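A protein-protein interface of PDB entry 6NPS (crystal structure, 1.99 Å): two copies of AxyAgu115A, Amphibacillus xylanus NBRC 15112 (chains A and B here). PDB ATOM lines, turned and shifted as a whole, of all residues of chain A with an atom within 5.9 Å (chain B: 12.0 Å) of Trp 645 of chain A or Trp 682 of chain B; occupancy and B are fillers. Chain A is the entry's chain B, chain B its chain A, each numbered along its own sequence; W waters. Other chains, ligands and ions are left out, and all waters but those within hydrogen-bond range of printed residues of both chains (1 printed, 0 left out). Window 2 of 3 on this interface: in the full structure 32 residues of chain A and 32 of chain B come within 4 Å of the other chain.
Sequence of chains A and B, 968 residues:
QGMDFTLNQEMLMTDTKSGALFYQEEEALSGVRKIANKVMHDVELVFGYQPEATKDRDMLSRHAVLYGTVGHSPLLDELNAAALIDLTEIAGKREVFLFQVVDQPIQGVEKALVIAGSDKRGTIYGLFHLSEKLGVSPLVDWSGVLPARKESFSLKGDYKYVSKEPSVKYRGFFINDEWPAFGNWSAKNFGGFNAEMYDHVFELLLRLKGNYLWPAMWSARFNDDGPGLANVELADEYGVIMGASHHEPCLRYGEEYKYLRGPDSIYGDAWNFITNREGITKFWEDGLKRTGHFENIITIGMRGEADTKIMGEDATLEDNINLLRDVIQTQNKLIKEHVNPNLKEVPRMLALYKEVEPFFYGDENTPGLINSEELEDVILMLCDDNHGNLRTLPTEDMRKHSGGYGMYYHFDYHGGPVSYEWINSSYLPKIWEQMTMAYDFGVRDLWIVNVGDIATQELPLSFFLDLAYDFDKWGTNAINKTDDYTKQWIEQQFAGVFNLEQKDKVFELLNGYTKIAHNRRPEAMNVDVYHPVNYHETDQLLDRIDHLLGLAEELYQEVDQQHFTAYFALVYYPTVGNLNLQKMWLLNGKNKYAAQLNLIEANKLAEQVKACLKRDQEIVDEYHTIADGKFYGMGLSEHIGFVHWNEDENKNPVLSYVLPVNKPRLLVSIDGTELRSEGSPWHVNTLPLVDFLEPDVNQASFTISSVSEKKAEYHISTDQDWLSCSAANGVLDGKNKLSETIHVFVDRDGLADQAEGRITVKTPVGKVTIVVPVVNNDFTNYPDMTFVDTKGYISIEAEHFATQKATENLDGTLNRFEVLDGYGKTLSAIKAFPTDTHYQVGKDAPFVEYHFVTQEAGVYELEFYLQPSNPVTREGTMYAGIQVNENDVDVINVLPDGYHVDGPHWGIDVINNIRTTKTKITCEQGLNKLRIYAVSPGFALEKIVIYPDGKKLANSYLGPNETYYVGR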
ATOM      1  N   HIS A 414     -28.449 -33.222  -8.004  1.00  0.00           N
ATOM      2  CA  HIS A 414     -27.395 -32.407  -8.604  1.00  0.00           C
ATOM      3  C   HIS A 414     -28.042 -31.616  -9.739  1.00  0.00           C
ATOM      4  O   HIS A 414     -28.307 -32.178 -10.802  1.00  0.00           O
ATOM      5  CB  HIS A 414     -26.295 -33.338  -9.100  1.00  0.00           C
ATOM      6  CG  HIS A 414     -25.089 -32.654  -9.670  1.00  0.00           C
ATOM      7  ND1 HIS A 414     -24.227 -31.894  -8.900  1.00  0.00           N
ATOM      8  CD2 HIS A 414     -24.559 -32.684 -10.920  1.00  0.00           C
ATOM      9  CE1 HIS A 414     -23.238 -31.454  -9.663  1.00  0.00           C
ATOM     10  NE2 HIS A 414     -23.415 -31.922 -10.889  1.00  0.00           N
ATOM     11  N   GLY A 415     -28.295 -30.329  -9.541  1.00  0.00           N
ATOM     12  CA  GLY A 415     -29.050 -29.583 -10.530  1.00  0.00           C
ATOM     13  C   GLY A 415     -29.646 -28.324  -9.896  1.00  0.00           C
ATOM     14  O   GLY A 415     -29.337 -27.969  -8.760  1.00  0.00           O
ATOM     15  N   GLY A 416     -30.502 -27.651 -10.651  1.00  0.00           N
ATOM     16  CA  GLY A 416     -31.017 -26.364 -10.195  1.00  0.00           C
ATOM     17  C   GLY A 416     -32.255 -26.453  -9.298  1.00  0.00           C
ATOM     18  O   GLY A 416     -32.914 -27.498  -9.210  1.00  0.00           O
ATOM     19  N   PRO A 417     -32.581 -25.357  -8.582  1.00  0.00           N
ATOM     20  CA  PRO A 417     -31.836 -24.088  -8.533  1.00  0.00           C
ATOM     21  C   PRO A 417     -30.529 -24.213  -7.745  1.00  0.00           C
ATOM     22  O   PRO A 417     -29.580 -23.520  -8.119  1.00  0.00           O
ATOM     23  CB  PRO A 417     -32.818 -23.109  -7.813  1.00  0.00           C
ATOM     24  CG  PRO A 417     -34.135 -23.762  -7.848  1.00  0.00           C
ATOM     25  CD  PRO A 417     -33.868 -25.274  -7.862  1.00  0.00           C
ATOM     26  N   VAL A 418     -30.465 -25.043  -6.705  1.00  0.00           N
ATOM     27  CA  VAL A 418     -29.228 -25.306  -5.954  1.00  0.00           C
ATOM     28  C   VAL A 418     -29.153 -26.803  -5.646  1.00  0.00           C
ATOM     29  O   VAL A 418     -30.113 -27.391  -5.147  1.00  0.00           O
ATOM     30  CB  VAL A 418     -29.144 -24.515  -4.626  1.00  0.00           C
ATOM     31  CG1 VAL A 418     -27.742 -24.728  -3.922  1.00  0.00           C
ATOM     32  CG2 VAL A 418     -29.431 -23.017  -4.842  1.00  0.00           C
ATOM     33  N   SER A 419     -27.998 -27.413  -5.888  1.00  0.00           N
ATOM     34  CA  SER A 419     -27.819 -28.842  -5.626  1.00  0.00           C
ATOM     35  C   SER A 419     -27.893 -29.119  -4.130  1.00  0.00           C
ATOM     36  O   SER A 419     -27.628 -28.234  -3.317  1.00  0.00           O
ATOM     37  CB  SER A 419     -26.432 -29.292  -6.152  1.00  0.00           C
ATOM     38  OG  SER A 419     -26.436 -29.239  -7.539  1.00  0.00           O
ATOM     39  N   PHE A 642     -22.761 -21.836  -1.987  1.00  0.00           N
ATOM     40  CA  PHE A 642     -22.947 -21.936  -3.423  1.00  0.00           C
ATOM     41  C   PHE A 642     -23.528 -20.639  -3.934  1.00  0.00           C
ATOM     42  O   PHE A 642     -24.356 -20.010  -3.269  1.00  0.00           O
ATOM     43  CB  PHE A 642     -23.898 -23.099  -3.789  1.00  0.00           C
ATOM     44  CG  PHE A 642     -23.239 -24.474  -3.833  1.00  0.00           C
ATOM     45  CD1 PHE A 642     -22.132 -24.772  -3.021  1.00  0.00           C
ATOM     46  CD2 PHE A 642     -23.767 -25.490  -4.642  1.00  0.00           C
ATOM     47  CE1 PHE A 642     -21.545 -26.075  -3.050  1.00  0.00           C
ATOM     48  CE2 PHE A 642     -23.200 -26.775  -4.659  1.00  0.00           C
ATOM     49  CZ  PHE A 642     -22.101 -27.078  -3.862  1.00  0.00           C
ATOM     50  N   VAL A 643     -23.044 -20.222  -5.082  1.00  0.00           N
ATOM     51  CA  VAL A 643     -23.569 -19.060  -5.802  1.00  0.00           C
ATOM     52  C   VAL A 643     -24.174 -19.466  -7.134  1.00  0.00           C
ATOM     53  O   VAL A 643     -24.721 -18.609  -7.847  1.00  0.00           O
ATOM     54  CB  VAL A 643     -22.479 -17.986  -6.031  1.00  0.00           C
ATOM     55  CG1 VAL A 643     -21.824 -17.586  -4.689  1.00  0.00           C
ATOM     56  CG2 VAL A 643     -21.434 -18.448  -7.058  1.00  0.00           C
ATOM     57  N   HIS A 644     -24.044 -20.736  -7.514  1.00  0.00           N
ATOM     58  CA  HIS A 644     -24.626 -21.312  -8.702  1.00  0.00           C
ATOM     59  C   HIS A 644     -25.352 -22.565  -8.280  1.00  0.00           C
ATOM     60  O   HIS A 644     -25.314 -22.945  -7.107  1.00  0.00           O
ATOM     61  CB  HIS A 644     -23.542 -21.668  -9.727  1.00  0.00           C
ATOM     62  CG  HIS A 644     -22.834 -20.465 -10.264  1.00  0.00           C
ATOM     63  ND1 HIS A 644     -23.516 -19.419 -10.853  1.00  0.00           N
ATOM     64  CD2 HIS A 644     -21.512 -20.162 -10.354  1.00  0.00           C
ATOM     65  CE1 HIS A 644     -22.646 -18.512 -11.273  1.00  0.00           C
ATOM     66  NE2 HIS A 644     -21.424 -18.943 -10.993  1.00  0.00           N
ATOM     67  N   TRP A 645     -25.982 -23.227  -9.254  1.00  0.00           N
ATOM     68  CA  TRP A 645     -26.634 -24.493  -8.955  1.00  0.00           C
ATOM     69  C   TRP A 645     -25.625 -25.520  -8.491  1.00  0.00           C
ATOM     70  O   TRP A 645     -25.983 -26.433  -7.746  1.00  0.00           O
ATOM     71  CB  TRP A 645     -27.376 -24.999 -10.190  1.00  0.00           C
ATOM     72  CG  TRP A 645     -26.495 -25.416 -11.340  1.00  0.00           C
ATOM     73  CD1 TRP A 645     -26.032 -24.615 -12.371  1.00  0.00           C
ATOM     74  CD2 TRP A 645     -25.979 -26.737 -11.593  1.00  0.00           C
ATOM     75  NE1 TRP A 645     -25.281 -25.373 -13.227  1.00  0.00           N
ATOM     76  CE2 TRP A 645     -25.217 -26.668 -12.766  1.00  0.00           C
ATOM     77  CE3 TRP A 645     -26.086 -27.962 -10.923  1.00  0.00           C
ATOM     78  CZ2 TRP A 645     -24.576 -27.810 -13.333  1.00  0.00           C
ATOM     79  CZ3 TRP A 645     -25.451 -29.095 -11.461  1.00  0.00           C
ATOM     80  CH2 TRP A 645     -24.691 -29.001 -12.659  1.00  0.00           C
ATOM     81  N   ASN A 646     -24.378 -25.443  -8.998  1.00  0.00           N
ATOM     82  CA  ASN A 646     -23.323 -26.376  -8.622  1.00  0.00           C
ATOM     83  C   ASN A 646     -22.240 -25.630  -7.836  1.00  0.00           C
ATOM     84  O   ASN A 646     -22.384 -24.458  -7.501  1.00  0.00           O
ATOM     85  CB  ASN A 646     -22.771 -27.094  -9.849  1.00  0.00           C
ATOM     86  CG  ASN A 646     -22.041 -26.180 -10.803  1.00  0.00           C
ATOM     87  OD1 ASN A 646     -22.121 -24.965 -10.695  1.00  0.00           O
ATOM     88  ND2 ASN A 646     -21.317 -26.772 -11.775  1.00  0.00           N
ATOM     89  N   GLU A 647     -21.173 -26.336  -7.495  1.00  0.00           N
ATOM     90  CA  GLU A 647     -20.166 -25.809  -6.589  1.00  0.00           C
ATOM     91  C   GLU A 647     -19.237 -24.793  -7.228  1.00  0.00           C
ATOM     92  O   GLU A 647     -18.428 -24.212  -6.501  1.00  0.00           O
ATOM     93  CB  GLU A 647     -19.319 -26.956  -6.053  1.00  0.00           C
ATOM     94  CG  GLU A 647     -18.598 -27.672  -7.198  1.00  0.00           C
ATOM     95  CD  GLU A 647     -17.470 -28.565  -6.732  1.00  0.00           C
ATOM     96  OE1 GLU A 647     -16.424 -28.033  -6.309  1.00  0.00           O
ATOM     97  OE2 GLU A 647     -17.633 -29.803  -6.790  1.00  0.00           O
ATOM     98  N   ASP A 648     -19.289 -24.591  -8.548  1.00  0.00           N
ATOM     99  CA  ASP A 648     -18.333 -23.694  -9.200  1.00  0.00           C
ATOM    100  C   ASP A 648     -18.407 -22.293  -8.581  1.00  0.00           C
ATOM    101  O   ASP A 648     -19.490 -21.719  -8.428  1.00  0.00           O
ATOM    102  CB  ASP A 648     -18.598 -23.598 -10.701  1.00  0.00           C
ATOM    103  CG  ASP A 648     -18.384 -24.943 -11.439  1.00  0.00           C
ATOM    104  OD1 ASP A 648     -17.703 -25.833 -10.900  1.00  0.00           O
ATOM    105  OD2 ASP A 648     -18.927 -25.112 -12.544  1.00  0.00           O
ATOM    106  N   LYS B 663     -10.517 -25.716  -2.798  1.00  0.00           N
ATOM    107  CA  LYS B 663      -9.867 -26.199  -4.024  1.00  0.00           C
ATOM    108  C   LYS B 663      -8.894 -25.161  -4.568  1.00  0.00           C
ATOM    109  O   LYS B 663      -9.082 -23.961  -4.359  1.00  0.00           O
ATOM    110  CB  LYS B 663     -10.905 -26.516  -5.090  1.00  0.00           C
ATOM    111  CG  LYS B 663     -11.618 -27.842  -4.889  1.00  0.00           C
ATOM    112  CD  LYS B 663     -12.606 -28.112  -6.010  1.00  0.00           C
ATOM    113  CE  LYS B 663     -13.543 -29.282  -5.657  1.00  0.00           C
ATOM    114  NZ  LYS B 663     -13.510 -29.654  -4.197  1.00  0.00           N
ATOM    115  N   ARG B 676     -14.654 -11.238 -15.212  1.00  0.00           N
ATOM    116  CA  ARG B 676     -13.819 -12.178 -14.475  1.00  0.00           C
ATOM    117  C   ARG B 676     -14.349 -13.589 -14.652  1.00  0.00           C
ATOM    118  O   ARG B 676     -15.511 -13.800 -15.018  1.00  0.00           O
ATOM    119  CB  ARG B 676     -13.742 -11.803 -12.977  1.00  0.00           C
ATOM    120  CG  ARG B 676     -15.070 -12.026 -12.188  1.00  0.00           C
ATOM    121  CD  ARG B 676     -15.359 -10.811 -11.358  1.00  0.00           C
ATOM    122  NE  ARG B 676     -16.742 -10.834 -10.938  1.00  0.00           N
ATOM    123  CZ  ARG B 676     -17.452  -9.762 -10.641  1.00  0.00           C
ATOM    124  NH1 ARG B 676     -16.894  -8.559 -10.695  1.00  0.00           N
ATOM    125  NH2 ARG B 676     -18.707  -9.912 -10.252  1.00  0.00           N
ATOM    126  N   SER B 677     -13.490 -14.563 -14.372  1.00  0.00           N
ATOM    127  CA  SER B 677     -13.974 -15.924 -14.546  1.00  0.00           C
ATOM    128  C   SER B 677     -13.052 -16.886 -13.809  1.00  0.00           C
ATOM    129  O   SER B 677     -11.837 -16.694 -13.788  1.00  0.00           O
ATOM    130  CB  SER B 677     -14.028 -16.311 -16.040  1.00  0.00           C
ATOM    131  OG  SER B 677     -14.290 -17.712 -16.197  1.00  0.00           O
ATOM    132  N   GLU B 678     -13.629 -17.949 -13.251  1.00  0.00           N
ATOM    133  CA  GLU B 678     -12.819 -19.053 -12.741  1.00  0.00           C
ATOM    134  C   GLU B 678     -12.661 -20.204 -13.724  1.00  0.00           C
ATOM    135  O   GLU B 678     -12.082 -21.236 -13.355  1.00  0.00           O
ATOM    136  CB  GLU B 678     -13.382 -19.571 -11.420  1.00  0.00           C
ATOM    137  CG  GLU B 678     -13.123 -18.600 -10.274  1.00  0.00           C
ATOM    138  CD  GLU B 678     -13.305 -19.186  -8.843  1.00  0.00           C
ATOM    139  OE1 GLU B 678     -13.160 -20.413  -8.628  1.00  0.00           O
ATOM    140  OE2 GLU B 678     -13.565 -18.383  -7.920  1.00  0.00           O
ATOM    141  N   GLY B 679     -13.159 -20.061 -14.952  1.00  0.00           N
ATOM    142  CA  GLY B 679     -12.952 -21.084 -15.961  1.00  0.00           C
ATOM    143  C   GLY B 679     -13.923 -22.239 -15.915  1.00  0.00           C
ATOM    144  O   GLY B 679     -13.622 -23.306 -16.453  1.00  0.00           O
ATOM    145  N   SER B 680     -15.102 -22.060 -15.299  1.00  0.00           N
ATOM    146  CA  SER B 680     -15.951 -23.238 -15.334  1.00  0.00           C
ATOM    147  C   SER B 680     -16.598 -23.389 -16.713  1.00  0.00           C
ATOM    148  O   SER B 680     -17.102 -22.406 -17.265  1.00  0.00           O
ATOM    149  CB  SER B 680     -17.080 -23.140 -14.273  1.00  0.00           C
ATOM    150  OG  SER B 680     -17.946 -24.233 -14.563  1.00  0.00           O
ATOM    151  N   PRO B 681     -16.660 -24.602 -17.265  1.00  0.00           N
ATOM    152  CA  PRO B 681     -17.457 -24.802 -18.487  1.00  0.00           C
ATOM    153  C   PRO B 681     -18.946 -24.574 -18.304  1.00  0.00           C
ATOM    154  O   PRO B 681     -19.669 -24.466 -19.311  1.00  0.00           O
ATOM    155  CB  PRO B 681     -17.204 -26.275 -18.847  1.00  0.00           C
ATOM    156  CG  PRO B 681     -16.225 -26.787 -17.860  1.00  0.00           C
ATOM    157  CD  PRO B 681     -16.165 -25.884 -16.721  1.00  0.00           C
ATOM    158  N   TRP B 682     -19.447 -24.564 -17.058  1.00  0.00           N
ATOM    159  CA  TRP B 682     -20.873 -24.435 -16.823  1.00  0.00           C
ATOM    160  C   TRP B 682     -21.334 -22.994 -16.753  1.00  0.00           C
ATOM    161  O   TRP B 682     -22.538 -22.756 -16.847  1.00  0.00           O
ATOM    162  CB  TRP B 682     -21.252 -25.147 -15.512  1.00  0.00           C
ATOM    163  CG  TRP B 682     -21.180 -26.645 -15.645  1.00  0.00           C
ATOM    164  CD1 TRP B 682     -20.188 -27.466 -15.187  1.00  0.00           C
ATOM    165  CD2 TRP B 682     -22.146 -27.486 -16.264  1.00  0.00           C
ATOM    166  NE1 TRP B 682     -20.484 -28.760 -15.474  1.00  0.00           N
ATOM    167  CE2 TRP B 682     -21.687 -28.811 -16.131  1.00  0.00           C
ATOM    168  CE3 TRP B 682     -23.362 -27.251 -16.901  1.00  0.00           C
ATOM    169  CZ2 TRP B 682     -22.392 -29.912 -16.636  1.00  0.00           C
ATOM    170  CZ3 TRP B 682     -24.074 -28.338 -17.399  1.00  0.00           C
ATOM    171  CH2 TRP B 682     -23.583 -29.660 -17.263  1.00  0.00           C
ATOM    172  N   HIS B 683     -20.418 -22.047 -16.564  1.00  0.00           N
ATOM    173  CA  HIS B 683     -20.748 -20.636 -16.377  1.00  0.00           C
ATOM    174  C   HIS B 683     -19.875 -19.819 -17.330  1.00  0.00           C
ATOM    175  O   HIS B 683     -19.383 -20.320 -18.340  1.00  0.00           O
ATOM    176  CB  HIS B 683     -20.601 -20.286 -14.889  1.00  0.00           C
ATOM    177  CG  HIS B 683     -21.317 -21.269 -14.019  1.00  0.00           C
ATOM    178  ND1 HIS B 683     -22.692 -21.291 -13.921  1.00  0.00           N
ATOM    179  CD2 HIS B 683     -20.873 -22.337 -13.314  1.00  0.00           C
ATOM    180  CE1 HIS B 683     -23.062 -22.303 -13.150  1.00  0.00           C
ATOM    181  NE2 HIS B 683     -21.978 -22.943 -12.757  1.00  0.00           N
ATOM    182  N   VAL B 684     -19.633 -18.556 -17.019  1.00  0.00           N
ATOM    183  CA  VAL B 684     -18.940 -17.701 -17.976  1.00  0.00           C
ATOM    184  C   VAL B 684     -17.442 -18.005 -17.948  1.00  0.00           C
ATOM    185  O   VAL B 684     -16.775 -17.955 -16.906  1.00  0.00           O
ATOM    186  CB  VAL B 684     -19.244 -16.210 -17.739  1.00  0.00           C
ATOM    187  CG1 VAL B 684     -18.427 -15.611 -16.614  1.00  0.00           C
ATOM    188  CG2 VAL B 684     -18.990 -15.409 -19.040  1.00  0.00           C
ATOM    189  N   ASN B 685     -16.909 -18.371 -19.094  1.00  0.00           N
ATOM    190  CA  ASN B 685     -15.493 -18.670 -19.175  1.00  0.00           C
ATOM    191  C   ASN B 685     -14.829 -18.004 -20.389  1.00  0.00           C
ATOM    192  O   ASN B 685     -13.702 -18.352 -20.721  1.00  0.00           O
ATOM    193  CB  ASN B 685     -15.320 -20.187 -19.213  1.00  0.00           C
ATOM    194  CG  ASN B 685     -16.106 -20.800 -20.342  1.00  0.00           C
ATOM    195  OD1 ASN B 685     -15.917 -20.430 -21.482  1.00  0.00           O
ATOM    196  ND2 ASN B 685     -17.013 -21.716 -20.034  1.00  0.00           N
ATOM    197  N   THR B 686     -15.517 -17.100 -21.083  1.00  0.00           N
ATOM    198  CA  THR B 686     -14.934 -16.331 -22.178  1.00  0.00           C
ATOM    199  C   THR B 686     -15.087 -14.857 -21.842  1.00  0.00           C
ATOM    200  O   THR B 686     -16.194 -14.406 -21.540  1.00  0.00           O
ATOM    201  CB  THR B 686     -15.594 -16.676 -23.528  1.00  0.00           C
ATOM    202  OG1 THR B 686     -15.461 -18.083 -23.777  1.00  0.00           O
ATOM    203  CG2 THR B 686     -14.917 -15.950 -24.690  1.00  0.00           C
ATOM    204  N   THR B 763      -6.217 -23.330 -15.649  1.00  0.00           N
ATOM    205  CA  THR B 763      -6.046 -23.321 -14.205  1.00  0.00           C
ATOM    206  C   THR B 763      -6.346 -24.722 -13.679  1.00  0.00           C
ATOM    207  O   THR B 763      -6.823 -25.572 -14.442  1.00  0.00           O
ATOM    208  CB  THR B 763      -6.982 -22.306 -13.547  1.00  0.00           C
ATOM    209  OG1 THR B 763      -8.305 -22.851 -13.545  1.00  0.00           O
ATOM    210  CG2 THR B 763      -6.960 -20.941 -14.279  1.00  0.00           C
ATOM    211  N   VAL B 765      -8.714 -25.948 -12.177  1.00  0.00           N
ATOM    212  CA  VAL B 765     -10.111 -26.355 -12.179  1.00  0.00           C
ATOM    213  C   VAL B 765     -10.836 -26.025 -13.476  1.00  0.00           C
ATOM    214  O   VAL B 765     -12.012 -26.382 -13.618  1.00  0.00           O
ATOM    215  CB  VAL B 765     -10.849 -25.747 -10.974  1.00  0.00           C
ATOM    216  CG1 VAL B 765     -10.066 -26.057  -9.694  1.00  0.00           C
ATOM    217  CG2 VAL B 765     -10.991 -24.247 -11.155  1.00  0.00           C
ATOM    218  N   GLY B 766     -10.176 -25.386 -14.445  1.00  0.00           N
ATOM    219  CA  GLY B 766     -10.885 -25.041 -15.668  1.00  0.00           C
ATOM    220  C   GLY B 766     -10.052 -24.254 -16.659  1.00  0.00           C
ATOM    221  O   GLY B 766      -8.825 -24.333 -16.633  1.00  0.00           O
ATOM    222  N   LYS B 767     -10.701 -23.457 -17.499  1.00  0.00           N
ATOM    223  CA  LYS B 767     -10.025 -22.799 -18.608  1.00  0.00           C
ATOM    224  C   LYS B 767     -10.766 -21.512 -18.924  1.00  0.00           C
ATOM    225  O   LYS B 767     -11.988 -21.542 -19.074  1.00  0.00           O
ATOM    226  CB  LYS B 767     -10.024 -23.721 -19.838  1.00  0.00           C
ATOM    227  CG  LYS B 767      -9.517 -23.056 -21.082  1.00  0.00           C
ATOM    228  CD  LYS B 767      -9.117 -24.084 -22.147  1.00  0.00           C
ATOM    229  CE  LYS B 767      -9.953 -25.325 -22.073  1.00  0.00           C
ATOM    230  NZ  LYS B 767     -10.043 -26.015 -23.391  1.00  0.00           N
ATOM    231  N   VAL B 768     -10.054 -20.401 -18.995  1.00  0.00           N
ATOM    232  CA  VAL B 768     -10.637 -19.104 -19.347  1.00  0.00           C
ATOM    233  C   VAL B 768     -10.099 -18.718 -20.719  1.00  0.00           C
ATOM    234  O   VAL B 768      -8.884 -18.776 -20.953  1.00  0.00           O
ATOM    235  CB  VAL B 768     -10.318 -18.028 -18.296  1.00  0.00           C
ATOM    236  CG1 VAL B 768     -10.842 -16.632 -18.748  1.00  0.00           C
ATOM    237  CG2 VAL B 768     -10.971 -18.407 -16.919  1.00  0.00           C
ATOM    238  N   THR B 769     -10.987 -18.338 -21.633  1.00  0.00           N
ATOM    239  CA  THR B 769     -10.558 -17.800 -22.918  1.00  0.00           C
ATOM    240  C   THR B 769     -10.705 -16.284 -22.892  1.00  0.00           C
ATOM    241  O   THR B 769     -11.740 -15.761 -22.461  1.00  0.00           O
ATOM    242  CB  THR B 769     -11.391 -18.450 -24.013  1.00  0.00           C
ATOM    243  OG1 THR B 769     -11.240 -19.863 -23.862  1.00  0.00           O
ATOM    244  CG2 THR B 769     -10.947 -18.049 -25.389  1.00  0.00           C
HETATM  245  O   HOH W   1     -24.817 -24.020 -15.770  1.00  0.00           O
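No position is printed for both chains.
OD1 of Asn 646 of chain A lies within hydrogen-bond range of NE2 of His 683 of chain B. The side-chain carboxylate of Asp 648 of chain A is in hydrogen-bond range of the side-chain hydroxyl of Ser 680 of chain B (2.4 Å). The side-chain carboxylate (OE1) of Glu 647 of chain A is in salt-bridge range of the side-chain amino group (NZ) of Lys 663 of chain B (3.9 Å).
OD2 of Asp 648 of chain A is in hydrogen-bond range of ND2 of Asn 646 of chain A (3.0 Å). The backbone carbonyl oxygen (O) of Trp 645 of chain A lies within hydrogen-bond range of the side-chain hydroxyl (OG) of Ser 419 of chain A (2.8 Å). OG of Ser 680 of chain B sits at hydrogen-bond distance from N of Trp 682 of chain B. The side-chain amide nitrogen (ND2) of Asn 685 of chain B lies within hydrogen-bond range of the backbone carbonyl oxygen (O) of His 683 of chain B. The side-chain amide nitrogen of Asn 685 of chain B lies within hydrogen-bond range of the backbone carbonyl oxygen of Ser 680 of chain B, 2.9 Å away.
His 683 of chain B touches His 644 of chain A. Trp 682 of chain B touches Trp 645 of chain A. CE1 of His 683 of chain B touches NE1 of Trp 645 of chain A, at 3.8 Å. CD1 of Trp 682 of chain B touches ND2 of Asn 646 of chain A (3.7 Å). Trp 682 of chain B touches Asp 648 of chain A. Asp 648 of chain A touches His 683 of chain B.
Water W1 lies within hydrogen-bond range of O of Trp 682 of chain B (2.8 Å) and NE1 of Trp 645 of chain A (2.9 Å).
Of the 13 printed residues of chain A, 5 touch a printed residue of chain B. Printed residues of chain B that touch a printed residue of chain A: Lys 663, Ser 680, Trp 682 and His 683. Along chain B the printed residues that touch a printed residue of chain A span positions 663 to 683. Among the printed residues, Asp or Glu carboxylates within 4 Å of a Lys or Arg side-chain nitrogen of the other chain: Glu 647 of chain A with Lys 663 of chain B.
Printed residues of chain B within 4 Å of Trp 645 of chain A: Trp 682 (3.8 Å) and His 683 (3.8 Å). Trp 682 of chain B touches just these residues of chain A: Trp 645 (3.8 Å), Asn 646 (3.7 Å) and Asp 648 (3.8 Å). Gly 416 of chain A touches none of the printed residues of chain B. No residue of chain B comes within 4 Å of Pro 417 of chain A. Val 418 of chain A touches none of the printed residues of chain B. No residue of chain B comes within 4 Å of Ser 419 of chain A. His 644 of chain A touches just one residue of chain B: His 683. Of chain B, only Trp 682 and His 683 come within 4 Å of Asn 646 of chain A. Of chain B, only Ser 680, Trp 682 and His 683 come within 4 Å of Asp 648 of chain A. Printed residues of chain B within 4 Å of Glu 647 of chain A: Lys 663 (3.2 Å). Of the printed residues of chain A, Lys 663 of chain B touches Glu 647 (3.2 Å). Printed residues of chain A within 4 Å of His 683 of chain B: His 644, Trp 645, Asn 646 and Asp 648. Gly 766 of chain B touches none of the printed residues of chain A. The nearest residue of chain B that does not touch Trp 645 of chain A is Ser 680 of chain B (7.5 Å). The nearest printed residue of chain A that does not touch Trp 682 of chain B is His 414 of chain A (6.2 Å). The nearest printed residue of chain B that does not touch Glu 647 of chain A is His 683 of chain B (6.3 Å).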
